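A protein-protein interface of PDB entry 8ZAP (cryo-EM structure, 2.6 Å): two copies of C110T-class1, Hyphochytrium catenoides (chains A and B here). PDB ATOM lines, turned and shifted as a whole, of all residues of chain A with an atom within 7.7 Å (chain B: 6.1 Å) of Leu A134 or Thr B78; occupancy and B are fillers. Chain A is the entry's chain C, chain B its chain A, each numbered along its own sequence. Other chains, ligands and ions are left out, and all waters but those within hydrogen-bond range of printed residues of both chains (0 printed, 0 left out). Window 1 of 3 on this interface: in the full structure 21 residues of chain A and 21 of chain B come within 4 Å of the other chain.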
ATOM      1  N   VAL A 106      -2.616  19.209   0.606  1.00  0.00           N
ATOM      2  CA  VAL A 106      -2.667  20.050  -0.587  1.00  0.00           C
ATOM      3  C   VAL A 106      -1.248  20.397  -1.015  1.00  0.00           C
ATOM      4  O   VAL A 106      -1.036  20.962  -2.094  1.00  0.00           O
ATOM      5  CB  VAL A 106      -3.503  21.330  -0.371  1.00  0.00           C
ATOM      6  CG1 VAL A 106      -4.804  21.022   0.350  1.00  0.00           C
ATOM      7  CG2 VAL A 106      -2.699  22.397   0.351  1.00  0.00           C
ATOM      8  N   PRO A 110      -0.752  16.521  -4.484  1.00  0.00           N
ATOM      9  CA  PRO A 110      -0.683  17.045  -5.855  1.00  0.00           C
ATOM     10  C   PRO A 110       0.689  16.870  -6.471  1.00  0.00           C
ATOM     11  O   PRO A 110       0.809  16.226  -7.519  1.00  0.00           O
ATOM     12  CB  PRO A 110      -1.050  18.526  -5.686  1.00  0.00           C
ATOM     13  CG  PRO A 110      -1.893  18.552  -4.485  1.00  0.00           C
ATOM     14  CD  PRO A 110      -1.291  17.537  -3.564  1.00  0.00           C
ATOM     15  N   ARG A 127      -3.620  18.885 -15.602  1.00  0.00           N
ATOM     16  CA  ARG A 127      -5.007  18.540 -15.302  1.00  0.00           C
ATOM     17  C   ARG A 127      -5.103  17.663 -14.060  1.00  0.00           C
ATOM     18  O   ARG A 127      -5.933  17.913 -13.180  1.00  0.00           O
ATOM     19  CB  ARG A 127      -5.643  17.833 -16.497  1.00  0.00           C
ATOM     20  CG  ARG A 127      -5.999  18.743 -17.649  1.00  0.00           C
ATOM     21  CD  ARG A 127      -6.870  18.022 -18.654  1.00  0.00           C
ATOM     22  NE  ARG A 127      -6.559  18.404 -20.025  1.00  0.00           N
ATOM     23  CZ  ARG A 127      -7.195  17.939 -21.092  1.00  0.00           C
ATOM     24  NH1 ARG A 127      -8.180  17.065 -20.980  1.00  0.00           N
ATOM     25  NH2 ARG A 127      -6.833  18.362 -22.298  1.00  0.00           N
ATOM     26  N   TYR A 128      -4.262  16.631 -13.977  1.00  0.00           N
ATOM     27  CA  TYR A 128      -4.261  15.760 -12.806  1.00  0.00           C
ATOM     28  C   TYR A 128      -3.843  16.520 -11.553  1.00  0.00           C
ATOM     29  O   TYR A 128      -4.442  16.346 -10.482  1.00  0.00           O
ATOM     30  CB  TYR A 128      -3.331  14.573 -13.050  1.00  0.00           C
ATOM     31  CG  TYR A 128      -3.918  13.508 -13.945  1.00  0.00           C
ATOM     32  CD1 TYR A 128      -5.194  13.018 -13.723  1.00  0.00           C
ATOM     33  CD2 TYR A 128      -3.200  13.000 -15.017  1.00  0.00           C
ATOM     34  CE1 TYR A 128      -5.737  12.046 -14.532  1.00  0.00           C
ATOM     35  CE2 TYR A 128      -3.737  12.027 -15.837  1.00  0.00           C
ATOM     36  CZ  TYR A 128      -5.006  11.554 -15.588  1.00  0.00           C
ATOM     37  OH  TYR A 128      -5.550  10.588 -16.395  1.00  0.00           O
ATOM     38  N   PHE A 129      -2.820  17.370 -11.676  1.00  0.00           N
ATOM     39  CA  PHE A 129      -2.369  18.172 -10.545  1.00  0.00           C
ATOM     40  C   PHE A 129      -3.505  19.026 -10.000  1.00  0.00           C
ATOM     41  O   PHE A 129      -3.757  19.048  -8.789  1.00  0.00           O
ATOM     42  CB  PHE A 129      -1.189  19.046 -10.975  1.00  0.00           C
ATOM     43  CG  PHE A 129      -0.671  19.955  -9.894  1.00  0.00           C
ATOM     44  CD1 PHE A 129      -1.192  21.229  -9.730  1.00  0.00           C
ATOM     45  CD2 PHE A 129       0.342  19.540  -9.051  1.00  0.00           C
ATOM     46  CE1 PHE A 129      -0.719  22.063  -8.739  1.00  0.00           C
ATOM     47  CE2 PHE A 129       0.820  20.371  -8.059  1.00  0.00           C
ATOM     48  CZ  PHE A 129       0.289  21.634  -7.904  1.00  0.00           C
ATOM     49  N   PHE A 130      -4.218  19.721 -10.887  1.00  0.00           N
ATOM     50  CA  PHE A 130      -5.278  20.613 -10.436  1.00  0.00           C
ATOM     51  C   PHE A 130      -6.496  19.845  -9.942  1.00  0.00           C
ATOM     52  O   PHE A 130      -7.182  20.308  -9.026  1.00  0.00           O
ATOM     53  CB  PHE A 130      -5.654  21.579 -11.555  1.00  0.00           C
ATOM     54  CG  PHE A 130      -4.841  22.837 -11.551  1.00  0.00           C
ATOM     55  CD1 PHE A 130      -5.058  23.814 -10.595  1.00  0.00           C
ATOM     56  CD2 PHE A 130      -3.834  23.031 -12.481  1.00  0.00           C
ATOM     57  CE1 PHE A 130      -4.303  24.970 -10.582  1.00  0.00           C
ATOM     58  CE2 PHE A 130      -3.078  24.184 -12.473  1.00  0.00           C
ATOM     59  CZ  PHE A 130      -3.312  25.154 -11.523  1.00  0.00           C
ATOM     60  N   ALA A 131      -6.773  18.671 -10.513  1.00  0.00           N
ATOM     61  CA  ALA A 131      -7.863  17.848 -10.002  1.00  0.00           C
ATOM     62  C   ALA A 131      -7.595  17.420  -8.566  1.00  0.00           C
ATOM     63  O   ALA A 131      -8.472  17.518  -7.700  1.00  0.00           O
ATOM     64  CB  ALA A 131      -8.068  16.631 -10.903  1.00  0.00           C
ATOM     65  N   VAL A 132      -6.371  16.961  -8.289  1.00  0.00           N
ATOM     66  CA  VAL A 132      -6.019  16.572  -6.926  1.00  0.00           C
ATOM     67  C   VAL A 132      -6.040  17.783  -5.997  1.00  0.00           C
ATOM     68  O   VAL A 132      -6.517  17.702  -4.856  1.00  0.00           O
ATOM     69  CB  VAL A 132      -4.653  15.866  -6.913  1.00  0.00           C
ATOM     70  CG1 VAL A 132      -4.273  15.480  -5.505  1.00  0.00           C
ATOM     71  CG2 VAL A 132      -4.698  14.637  -7.792  1.00  0.00           C
ATOM     72  N   PHE A 133      -5.519  18.917  -6.470  1.00  0.00           N
ATOM     73  CA  PHE A 133      -5.532  20.155  -5.697  1.00  0.00           C
ATOM     74  C   PHE A 133      -6.948  20.527  -5.271  1.00  0.00           C
ATOM     75  O   PHE A 133      -7.211  20.803  -4.093  1.00  0.00           O
ATOM     76  CB  PHE A 133      -4.909  21.263  -6.549  1.00  0.00           C
ATOM     77  CG  PHE A 133      -4.530  22.494  -5.785  1.00  0.00           C
ATOM     78  CD1 PHE A 133      -3.476  22.476  -4.890  1.00  0.00           C
ATOM     79  CD2 PHE A 133      -5.206  23.684  -5.993  1.00  0.00           C
ATOM     80  CE1 PHE A 133      -3.119  23.614  -4.200  1.00  0.00           C
ATOM     81  CE2 PHE A 133      -4.851  24.825  -5.306  1.00  0.00           C
ATOM     82  CZ  PHE A 133      -3.805  24.791  -4.411  1.00  0.00           C
ATOM     83  N   LEU A 134      -7.880  20.526  -6.226  1.00  0.00           N
ATOM     84  CA  LEU A 134      -9.252  20.918  -5.933  1.00  0.00           C
ATOM     85  C   LEU A 134      -9.949  19.893  -5.050  1.00  0.00           C
ATOM     86  O   LEU A 134     -10.740  20.262  -4.178  1.00  0.00           O
ATOM     87  CB  LEU A 134     -10.022  21.130  -7.234  1.00  0.00           C
ATOM     88  CG  LEU A 134      -9.660  22.431  -7.949  1.00  0.00           C
ATOM     89  CD1 LEU A 134     -10.694  22.788  -8.999  1.00  0.00           C
ATOM     90  CD2 LEU A 134      -9.508  23.552  -6.937  1.00  0.00           C
ATOM     91  N   THR A 135      -9.670  18.604  -5.257  1.00  0.00           N
ATOM     92  CA  THR A 135     -10.245  17.580  -4.390  1.00  0.00           C
ATOM     93  C   THR A 135      -9.815  17.784  -2.943  1.00  0.00           C
ATOM     94  O   THR A 135     -10.641  17.725  -2.019  1.00  0.00           O
ATOM     95  CB  THR A 135      -9.825  16.196  -4.884  1.00  0.00           C
ATOM     96  OG1 THR A 135     -10.126  16.073  -6.280  1.00  0.00           O
ATOM     97  CG2 THR A 135     -10.549  15.114  -4.122  1.00  0.00           C
ATOM     98  N   LEU A 136      -8.527  18.047  -2.727  1.00  0.00           N
ATOM     99  CA  LEU A 136      -8.032  18.252  -1.373  1.00  0.00           C
ATOM    100  C   LEU A 136      -8.558  19.538  -0.754  1.00  0.00           C
ATOM    101  O   LEU A 136      -8.830  19.573   0.449  1.00  0.00           O
ATOM    102  CB  LEU A 136      -6.509  18.256  -1.373  1.00  0.00           C
ATOM    103  CG  LEU A 136      -5.912  16.899  -1.718  1.00  0.00           C
ATOM    104  CD1 LEU A 136      -4.473  17.093  -2.085  1.00  0.00           C
ATOM    105  CD2 LEU A 136      -6.059  15.930  -0.560  1.00  0.00           C
ATOM    106  N   TRP A 137      -8.705  20.600  -1.545  1.00  0.00           N
ATOM    107  CA  TRP A 137      -9.295  21.820  -1.008  1.00  0.00           C
ATOM    108  C   TRP A 137     -10.772  21.658  -0.680  1.00  0.00           C
ATOM    109  O   TRP A 137     -11.244  22.243   0.301  1.00  0.00           O
ATOM    110  CB  TRP A 137      -9.086  22.979  -1.979  1.00  0.00           C
ATOM    111  CG  TRP A 137      -7.794  23.678  -1.737  1.00  0.00           C
ATOM    112  CD1 TRP A 137      -6.723  23.727  -2.573  1.00  0.00           C
ATOM    113  CD2 TRP A 137      -7.423  24.408  -0.563  1.00  0.00           C
ATOM    114  NE1 TRP A 137      -5.710  24.452  -2.000  1.00  0.00           N
ATOM    115  CE2 TRP A 137      -6.114  24.882  -0.765  1.00  0.00           C
ATOM    116  CE3 TRP A 137      -8.072  24.714   0.636  1.00  0.00           C
ATOM    117  CZ2 TRP A 137      -5.440  25.643   0.186  1.00  0.00           C
ATOM    118  CZ3 TRP A 137      -7.404  25.469   1.578  1.00  0.00           C
ATOM    119  CH2 TRP A 137      -6.101  25.926   1.348  1.00  0.00           C
ATOM    120  N   CYS A 138     -11.506  20.869  -1.464  1.00  0.00           N
ATOM    121  CA  CYS A 138     -12.873  20.518  -1.102  1.00  0.00           C
ATOM    122  C   CYS A 138     -12.919  19.728   0.198  1.00  0.00           C
ATOM    123  O   CYS A 138     -13.818  19.943   1.016  1.00  0.00           O
ATOM    124  CB  CYS A 138     -13.527  19.719  -2.228  1.00  0.00           C
ATOM    125  SG  CYS A 138     -13.803  20.643  -3.748  1.00  0.00           S
ATOM    126  N   GLY A 139     -11.965  18.817   0.404  1.00  0.00           N
ATOM    127  CA  GLY A 139     -11.869  18.138   1.686  1.00  0.00           C
ATOM    128  C   GLY A 139     -11.570  19.059   2.850  1.00  0.00           C
ATOM    129  O   GLY A 139     -12.143  18.900   3.934  1.00  0.00           O
ATOM    130  N   VAL A 140     -10.670  20.023   2.650  1.00  0.00           N
ATOM    131  CA  VAL A 140     -10.384  21.010   3.688  1.00  0.00           C
ATOM    132  C   VAL A 140     -11.638  21.809   4.020  1.00  0.00           C
ATOM    133  O   VAL A 140     -11.967  22.025   5.195  1.00  0.00           O
ATOM    134  CB  VAL A 140      -9.232  21.930   3.241  1.00  0.00           C
ATOM    135  CG1 VAL A 140      -9.084  23.110   4.190  1.00  0.00           C
ATOM    136  CG2 VAL A 140      -7.936  21.151   3.143  1.00  0.00           C
ATOM    137  N   ALA A 141     -12.361  22.251   2.990  1.00  0.00           N
ATOM    138  CA  ALA A 141     -13.604  22.981   3.198  1.00  0.00           C
ATOM    139  C   ALA A 141     -14.638  22.139   3.929  1.00  0.00           C
ATOM    140  O   ALA A 141     -15.362  22.658   4.786  1.00  0.00           O
ATOM    141  CB  ALA A 141     -14.154  23.449   1.855  1.00  0.00           C
ATOM    142  N   TYR A 153     -19.504  20.113   0.242  1.00  0.00           N
ATOM    143  CA  TYR A 153     -18.087  20.207  -0.085  1.00  0.00           C
ATOM    144  C   TYR A 153     -17.489  18.837  -0.354  1.00  0.00           C
ATOM    145  O   TYR A 153     -16.836  18.641  -1.387  1.00  0.00           O
ATOM    146  CB  TYR A 153     -17.326  20.887   1.051  1.00  0.00           C
ATOM    147  CG  TYR A 153     -17.434  22.392   1.067  1.00  0.00           C
ATOM    148  CD1 TYR A 153     -16.991  23.151  -0.006  1.00  0.00           C
ATOM    149  CD2 TYR A 153     -17.975  23.052   2.158  1.00  0.00           C
ATOM    150  CE1 TYR A 153     -17.082  24.527   0.011  1.00  0.00           C
ATOM    151  CE2 TYR A 153     -18.072  24.425   2.183  1.00  0.00           C
ATOM    152  CZ  TYR A 153     -17.625  25.159   1.108  1.00  0.00           C
ATOM    153  OH  TYR A 153     -17.725  26.530   1.135  1.00  0.00           O
ATOM    154  N   LEU A 156     -18.607  17.809  -3.615  1.00  0.00           N
ATOM    155  CA  LEU A 156     -17.826  18.519  -4.616  1.00  0.00           C
ATOM    156  C   LEU A 156     -16.483  17.835  -4.828  1.00  0.00           C
ATOM    157  O   LEU A 156     -16.080  17.588  -5.971  1.00  0.00           O
ATOM    158  CB  LEU A 156     -17.642  19.977  -4.195  1.00  0.00           C
ATOM    159  CG  LEU A 156     -17.037  20.953  -5.206  1.00  0.00           C
ATOM    160  CD1 LEU A 156     -17.850  20.976  -6.489  1.00  0.00           C
ATOM    161  CD2 LEU A 156     -16.950  22.343  -4.599  1.00  0.00           C
ATOM    162  N   GLY A 157     -15.803  17.472  -3.736  1.00  0.00           N
ATOM    163  CA  GLY A 157     -14.586  16.698  -3.863  1.00  0.00           C
ATOM    164  C   GLY A 157     -14.791  15.362  -4.533  1.00  0.00           C
ATOM    165  O   GLY A 157     -13.966  14.962  -5.361  1.00  0.00           O
ATOM    166  N   CYS A 158     -15.889  14.682  -4.219  1.00  0.00           N
ATOM    167  CA  CYS A 158     -16.230  13.440  -4.889  1.00  0.00           C
ATOM    168  C   CYS A 158     -16.556  13.649  -6.358  1.00  0.00           C
ATOM    169  O   CYS A 158     -16.464  12.698  -7.140  1.00  0.00           O
ATOM    170  CB  CYS A 158     -17.410  12.767  -4.183  1.00  0.00           C
ATOM    171  SG  CYS A 158     -16.956  11.920  -2.657  1.00  0.00           S
ATOM    172  N   TRP A 160     -14.729  15.718  -8.091  1.00  0.00           N
ATOM    173  CA  TRP A 160     -13.402  15.939  -8.647  1.00  0.00           C
ATOM    174  C   TRP A 160     -12.497  14.727  -8.531  1.00  0.00           C
ATOM    175  O   TRP A 160     -11.568  14.587  -9.326  1.00  0.00           O
ATOM    176  CB  TRP A 160     -12.729  17.130  -7.954  1.00  0.00           C
ATOM    177  CG  TRP A 160     -12.946  18.428  -8.656  1.00  0.00           C
ATOM    178  CD1 TRP A 160     -13.745  19.454  -8.250  1.00  0.00           C
ATOM    179  CD2 TRP A 160     -12.355  18.845  -9.891  1.00  0.00           C
ATOM    180  NE1 TRP A 160     -13.692  20.483  -9.155  1.00  0.00           N
ATOM    181  CE2 TRP A 160     -12.843  20.135 -10.173  1.00  0.00           C
ATOM    182  CE3 TRP A 160     -11.459  18.253 -10.786  1.00  0.00           C
ATOM    183  CZ2 TRP A 160     -12.469  20.841 -11.310  1.00  0.00           C
ATOM    184  CZ3 TRP A 160     -11.088  18.957 -11.914  1.00  0.00           C
ATOM    185  CH2 TRP A 160     -11.592  20.238 -12.167  1.00  0.00           C
ATOM    186  N   PHE A 161     -12.752  13.848  -7.560  1.00  0.00           N
ATOM    187  CA  PHE A 161     -11.925  12.662  -7.384  1.00  0.00           C
ATOM    188  C   PHE A 161     -12.399  11.507  -8.256  1.00  0.00           C
ATOM    189  O   PHE A 161     -11.577  10.789  -8.833  1.00  0.00           O
ATOM    190  CB  PHE A 161     -11.914  12.242  -5.916  1.00  0.00           C
ATOM    191  CG  PHE A 161     -10.937  11.149  -5.609  1.00  0.00           C
ATOM    192  CD1 PHE A 161     -11.368   9.950  -5.066  1.00  0.00           C
ATOM    193  CD2 PHE A 161      -9.589  11.313  -5.868  1.00  0.00           C
ATOM    194  CE1 PHE A 161     -10.473   8.940  -4.787  1.00  0.00           C
ATOM    195  CE2 PHE A 161      -8.691  10.307  -5.591  1.00  0.00           C
ATOM    196  CZ  PHE A 161      -9.134   9.118  -5.051  1.00  0.00           C
ATOM    197  N   CYS B  32     -21.394  28.718 -11.464  1.00  0.00           N
ATOM    198  CA  CYS B  32     -20.598  27.507 -11.332  1.00  0.00           C
ATOM    199  C   CYS B  32     -20.899  26.538 -12.463  1.00  0.00           C
ATOM    200  O   CYS B  32     -19.989  26.034 -13.127  1.00  0.00           O
ATOM    201  CB  CYS B  32     -20.869  26.847  -9.978  1.00  0.00           C
ATOM    202  SG  CYS B  32     -20.573  25.065  -9.958  1.00  0.00           S
ATOM    203  N   ALA B  36     -17.980  25.915 -15.203  1.00  0.00           N
ATOM    204  CA  ALA B  36     -17.453  24.556 -15.180  1.00  0.00           C
ATOM    205  C   ALA B  36     -17.770  23.813 -16.473  1.00  0.00           C
ATOM    206  O   ALA B  36     -16.920  23.083 -16.995  1.00  0.00           O
ATOM    207  CB  ALA B  36     -18.004  23.800 -13.972  1.00  0.00           C
ATOM    208  N   ILE B  71      -8.729  24.423 -17.413  1.00  0.00           N
ATOM    209  CA  ILE B  71      -8.396  24.226 -16.005  1.00  0.00           C
ATOM    210  C   ILE B  71      -8.805  25.441 -15.184  1.00  0.00           C
ATOM    211  O   ILE B  71      -9.363  25.310 -14.089  1.00  0.00           O
ATOM    212  CB  ILE B  71      -6.896  23.912 -15.854  1.00  0.00           C
ATOM    213  CG1 ILE B  71      -6.633  22.428 -16.105  1.00  0.00           C
ATOM    214  CG2 ILE B  71      -6.393  24.317 -14.480  1.00  0.00           C
ATOM    215  CD1 ILE B  71      -5.201  22.121 -16.460  1.00  0.00           C
ATOM    216  N   CYS B  73     -11.136  27.662 -15.991  1.00  0.00           N
ATOM    217  CA  CYS B  73     -12.592  27.723 -15.948  1.00  0.00           C
ATOM    218  C   CYS B  73     -13.171  26.706 -14.972  1.00  0.00           C
ATOM    219  O   CYS B  73     -14.122  27.018 -14.251  1.00  0.00           O
ATOM    220  CB  CYS B  73     -13.168  27.522 -17.347  1.00  0.00           C
ATOM    221  SG  CYS B  73     -13.444  29.056 -18.242  1.00  0.00           S
ATOM    222  N   LEU B  74     -12.609  25.498 -14.919  1.00  0.00           N
ATOM    223  CA  LEU B  74     -13.080  24.502 -13.965  1.00  0.00           C
ATOM    224  C   LEU B  74     -12.761  24.887 -12.527  1.00  0.00           C
ATOM    225  O   LEU B  74     -13.576  24.644 -11.633  1.00  0.00           O
ATOM    226  CB  LEU B  74     -12.476  23.139 -14.294  1.00  0.00           C
ATOM    227  CG  LEU B  74     -13.245  22.346 -15.349  1.00  0.00           C
ATOM    228  CD1 LEU B  74     -12.315  21.407 -16.089  1.00  0.00           C
ATOM    229  CD2 LEU B  74     -14.392  21.585 -14.715  1.00  0.00           C
ATOM    230  N   LEU B  75     -11.593  25.483 -12.283  1.00  0.00           N
ATOM    231  CA  LEU B  75     -11.266  25.966 -10.946  1.00  0.00           C
ATOM    232  C   LEU B  75     -12.195  27.098 -10.526  1.00  0.00           C
ATOM    233  O   LEU B  75     -12.638  27.150  -9.372  1.00  0.00           O
ATOM    234  CB  LEU B  75      -9.801  26.402 -10.900  1.00  0.00           C
ATOM    235  CG  LEU B  75      -9.352  27.408  -9.838  1.00  0.00           C
ATOM    236  CD1 LEU B  75      -9.081  26.721  -8.516  1.00  0.00           C
ATOM    237  CD2 LEU B  75      -8.108  28.133 -10.312  1.00  0.00           C
ATOM    238  N   CYS B  76     -12.513  28.006 -11.451  1.00  0.00           N
ATOM    239  CA  CYS B  76     -13.466  29.069 -11.156  1.00  0.00           C
ATOM    240  C   CYS B  76     -14.859  28.507 -10.895  1.00  0.00           C
ATOM    241  O   CYS B  76     -15.569  28.986 -10.005  1.00  0.00           O
ATOM    242  CB  CYS B  76     -13.493  30.079 -12.304  1.00  0.00           C
ATOM    243  SG  CYS B  76     -14.710  31.403 -12.130  1.00  0.00           S
ATOM    244  N   GLY B  77     -15.268  27.489 -11.655  1.00  0.00           N
ATOM    245  CA  GLY B  77     -16.555  26.860 -11.408  1.00  0.00           C
ATOM    246  C   GLY B  77     -16.614  26.150 -10.068  1.00  0.00           C
ATOM    247  O   GLY B  77     -17.638  26.186  -9.382  1.00  0.00           O
ATOM    248  N   THR B  78     -15.523  25.492  -9.678  1.00  0.00           N
ATOM    249  CA  THR B  78     -15.456  24.882  -8.355  1.00  0.00           C
ATOM    250  C   THR B  78     -15.512  25.929  -7.250  1.00  0.00           C
ATOM    251  O   THR B  78     -16.208  25.736  -6.243  1.00  0.00           O
ATOM    252  CB  THR B  78     -14.184  24.045  -8.228  1.00  0.00           C
ATOM    253  OG1 THR B  78     -13.990  23.290  -9.430  1.00  0.00           O
ATOM    254  CG2 THR B  78     -14.281  23.093  -7.049  1.00  0.00           C
ATOM    255  N   MET B  79     -14.798  27.043  -7.418  1.00  0.00           N
ATOM    256  CA  MET B  79     -14.862  28.097  -6.415  1.00  0.00           C
ATOM    257  C   MET B  79     -16.243  28.735  -6.370  1.00  0.00           C
ATOM    258  O   MET B  79     -16.684  29.182  -5.312  1.00  0.00           O
ATOM    259  CB  MET B  79     -13.789  29.155  -6.659  1.00  0.00           C
ATOM    260  CG  MET B  79     -12.373  28.641  -6.532  1.00  0.00           C
ATOM    261  SD  MET B  79     -11.184  29.982  -6.642  1.00  0.00           S
ATOM    262  CE  MET B  79     -11.566  30.601  -8.270  1.00  0.00           C
ATOM    263  N   TYR B  80     -16.952  28.773  -7.499  1.00  0.00           N
ATOM    264  CA  TYR B  80     -18.319  29.278  -7.476  1.00  0.00           C
ATOM    265  C   TYR B  80     -19.292  28.287  -6.856  1.00  0.00           C
ATOM    266  O   TYR B  80     -20.281  28.709  -6.255  1.00  0.00           O
ATOM    267  CB  TYR B  80     -18.777  29.663  -8.882  1.00  0.00           C
ATOM    268  CG  TYR B  80     -18.575  31.131  -9.163  1.00  0.00           C
ATOM    269  CD1 TYR B  80     -17.422  31.587  -9.780  1.00  0.00           C
ATOM    270  CD2 TYR B  80     -19.524  32.066  -8.774  1.00  0.00           C
ATOM    271  CE1 TYR B  80     -17.228  32.926 -10.023  1.00  0.00           C
ATOM    272  CE2 TYR B  80     -19.337  33.411  -9.013  1.00  0.00           C
ATOM    273  CZ  TYR B  80     -18.188  33.834  -9.638  1.00  0.00           C
ATOM    274  OH  TYR B  80     -17.990  35.171  -9.880  1.00  0.00           O
ATOM    275  N   ALA B  81     -19.033  26.986  -6.978  1.00  0.00           N
ATOM    276  CA  ALA B  81     -19.797  26.015  -6.202  1.00  0.00           C
ATOM    277  C   ALA B  81     -19.582  26.228  -4.709  1.00  0.00           C
ATOM    278  O   ALA B  81     -20.537  26.197  -3.924  1.00  0.00           O
ATOM    279  CB  ALA B  81     -19.409  24.593  -6.604  1.00  0.00           C
ATOM    280  N   ALA B  82     -18.332  26.464  -4.306  1.00  0.00           N
ATOM    281  CA  ALA B  82     -18.048  26.790  -2.912  1.00  0.00           C
ATOM    282  C   ALA B  82     -18.719  28.094  -2.488  1.00  0.00           C
ATOM    283  O   ALA B  82     -19.216  28.199  -1.362  1.00  0.00           O
ATOM    284  CB  ALA B  82     -16.540  26.870  -2.690  1.00  0.00           C
ATOM    285  N   LYS B  83     -18.732  29.095  -3.370  1.00  0.00           N
ATOM    286  CA  LYS B  83     -19.412  30.354  -3.090  1.00  0.00           C
ATOM    287  C   LYS B  83     -20.909  30.159  -2.915  1.00  0.00           C
ATOM    288  O   LYS B  83     -21.517  30.790  -2.046  1.00  0.00           O
ATOM    289  CB  LYS B  83     -19.155  31.351  -4.218  1.00  0.00           C
ATOM    290  CG  LYS B  83     -17.754  31.914  -4.272  1.00  0.00           C
ATOM    291  CD  LYS B  83     -17.551  32.687  -5.563  1.00  0.00           C
ATOM    292  CE  LYS B  83     -16.104  33.085  -5.752  1.00  0.00           C
ATOM    293  NZ  LYS B  83     -15.904  34.529  -5.466  1.00  0.00           N
ATOM    294  N   LEU B  97     -15.362  31.599   0.166  1.00  0.00           N
ATOM    295  CA  LEU B  97     -14.659  32.155  -0.978  1.00  0.00           C
ATOM    296  C   LEU B  97     -15.274  33.468  -1.434  1.00  0.00           C
ATOM    297  O   LEU B  97     -14.846  34.032  -2.446  1.00  0.00           O
ATOM    298  CB  LEU B  97     -14.634  31.141  -2.122  1.00  0.00           C
ATOM    299  CG  LEU B  97     -13.734  29.934  -1.860  1.00  0.00           C
ATOM    300  CD1 LEU B  97     -13.604  29.082  -3.098  1.00  0.00           C
ATOM    301  CD2 LEU B  97     -12.366  30.377  -1.372  1.00  0.00           C
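The side-chain hydroxyl of Thr B78 sits at hydrogen-bond distance from the indole nitrogen of Trp A160, 2.8 Å away. The backbone carbonyl oxygen (O) of Ala B82 lies within hydrogen-bond range of the side-chain hydroxyl (OH) of Tyr A153.
O of Leu A134 lies within hydrogen-bond range of SG of Cys A138 (3.1 Å). O of Leu B74 is in hydrogen-bond range of OG1 of Thr B78 (2.6 Å).
Among the printed residues, merely in contact across the chains: Leu A134 with Thr B78, Phe A130 with Ile B71, Leu A134 with Leu B75, Arg A127 with Ile B71, Leu A156 with Thr B78, Trp A160 with Leu B74 and Leu A156 with Ala B81.
Leu A134 touches just these residues of chain B: Leu B75 and Thr B78. Of chain A, only Leu A134, Leu A156 and Trp A160 come within 4 Å of Thr B78. Gly B77 touches none of the printed residues of chain A. Printed residues of chain B within 4 Å of Leu A156: Thr B78 (3.7 Å) and Ala B81 (3.9 Å). Of the printed residues of chain B, Phe A130 touches Ile B71. Of the printed residues of chain A, Leu B75 touches Leu A134 (3.6 Å). Of the printed residues of chain A, Leu B74 touches Trp A160. Cys B32 touches none of the printed residues of chain A.
Printed residues of chain A that touch a printed residue of chain B: Arg A127, Phe A130, Leu A134, Tyr A153, Leu A156 and Trp A160.
No position is printed for both chains. Of the 9 pairs that touch across the chains among the printed residues, none has its exchanged pair printed and touching as well.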
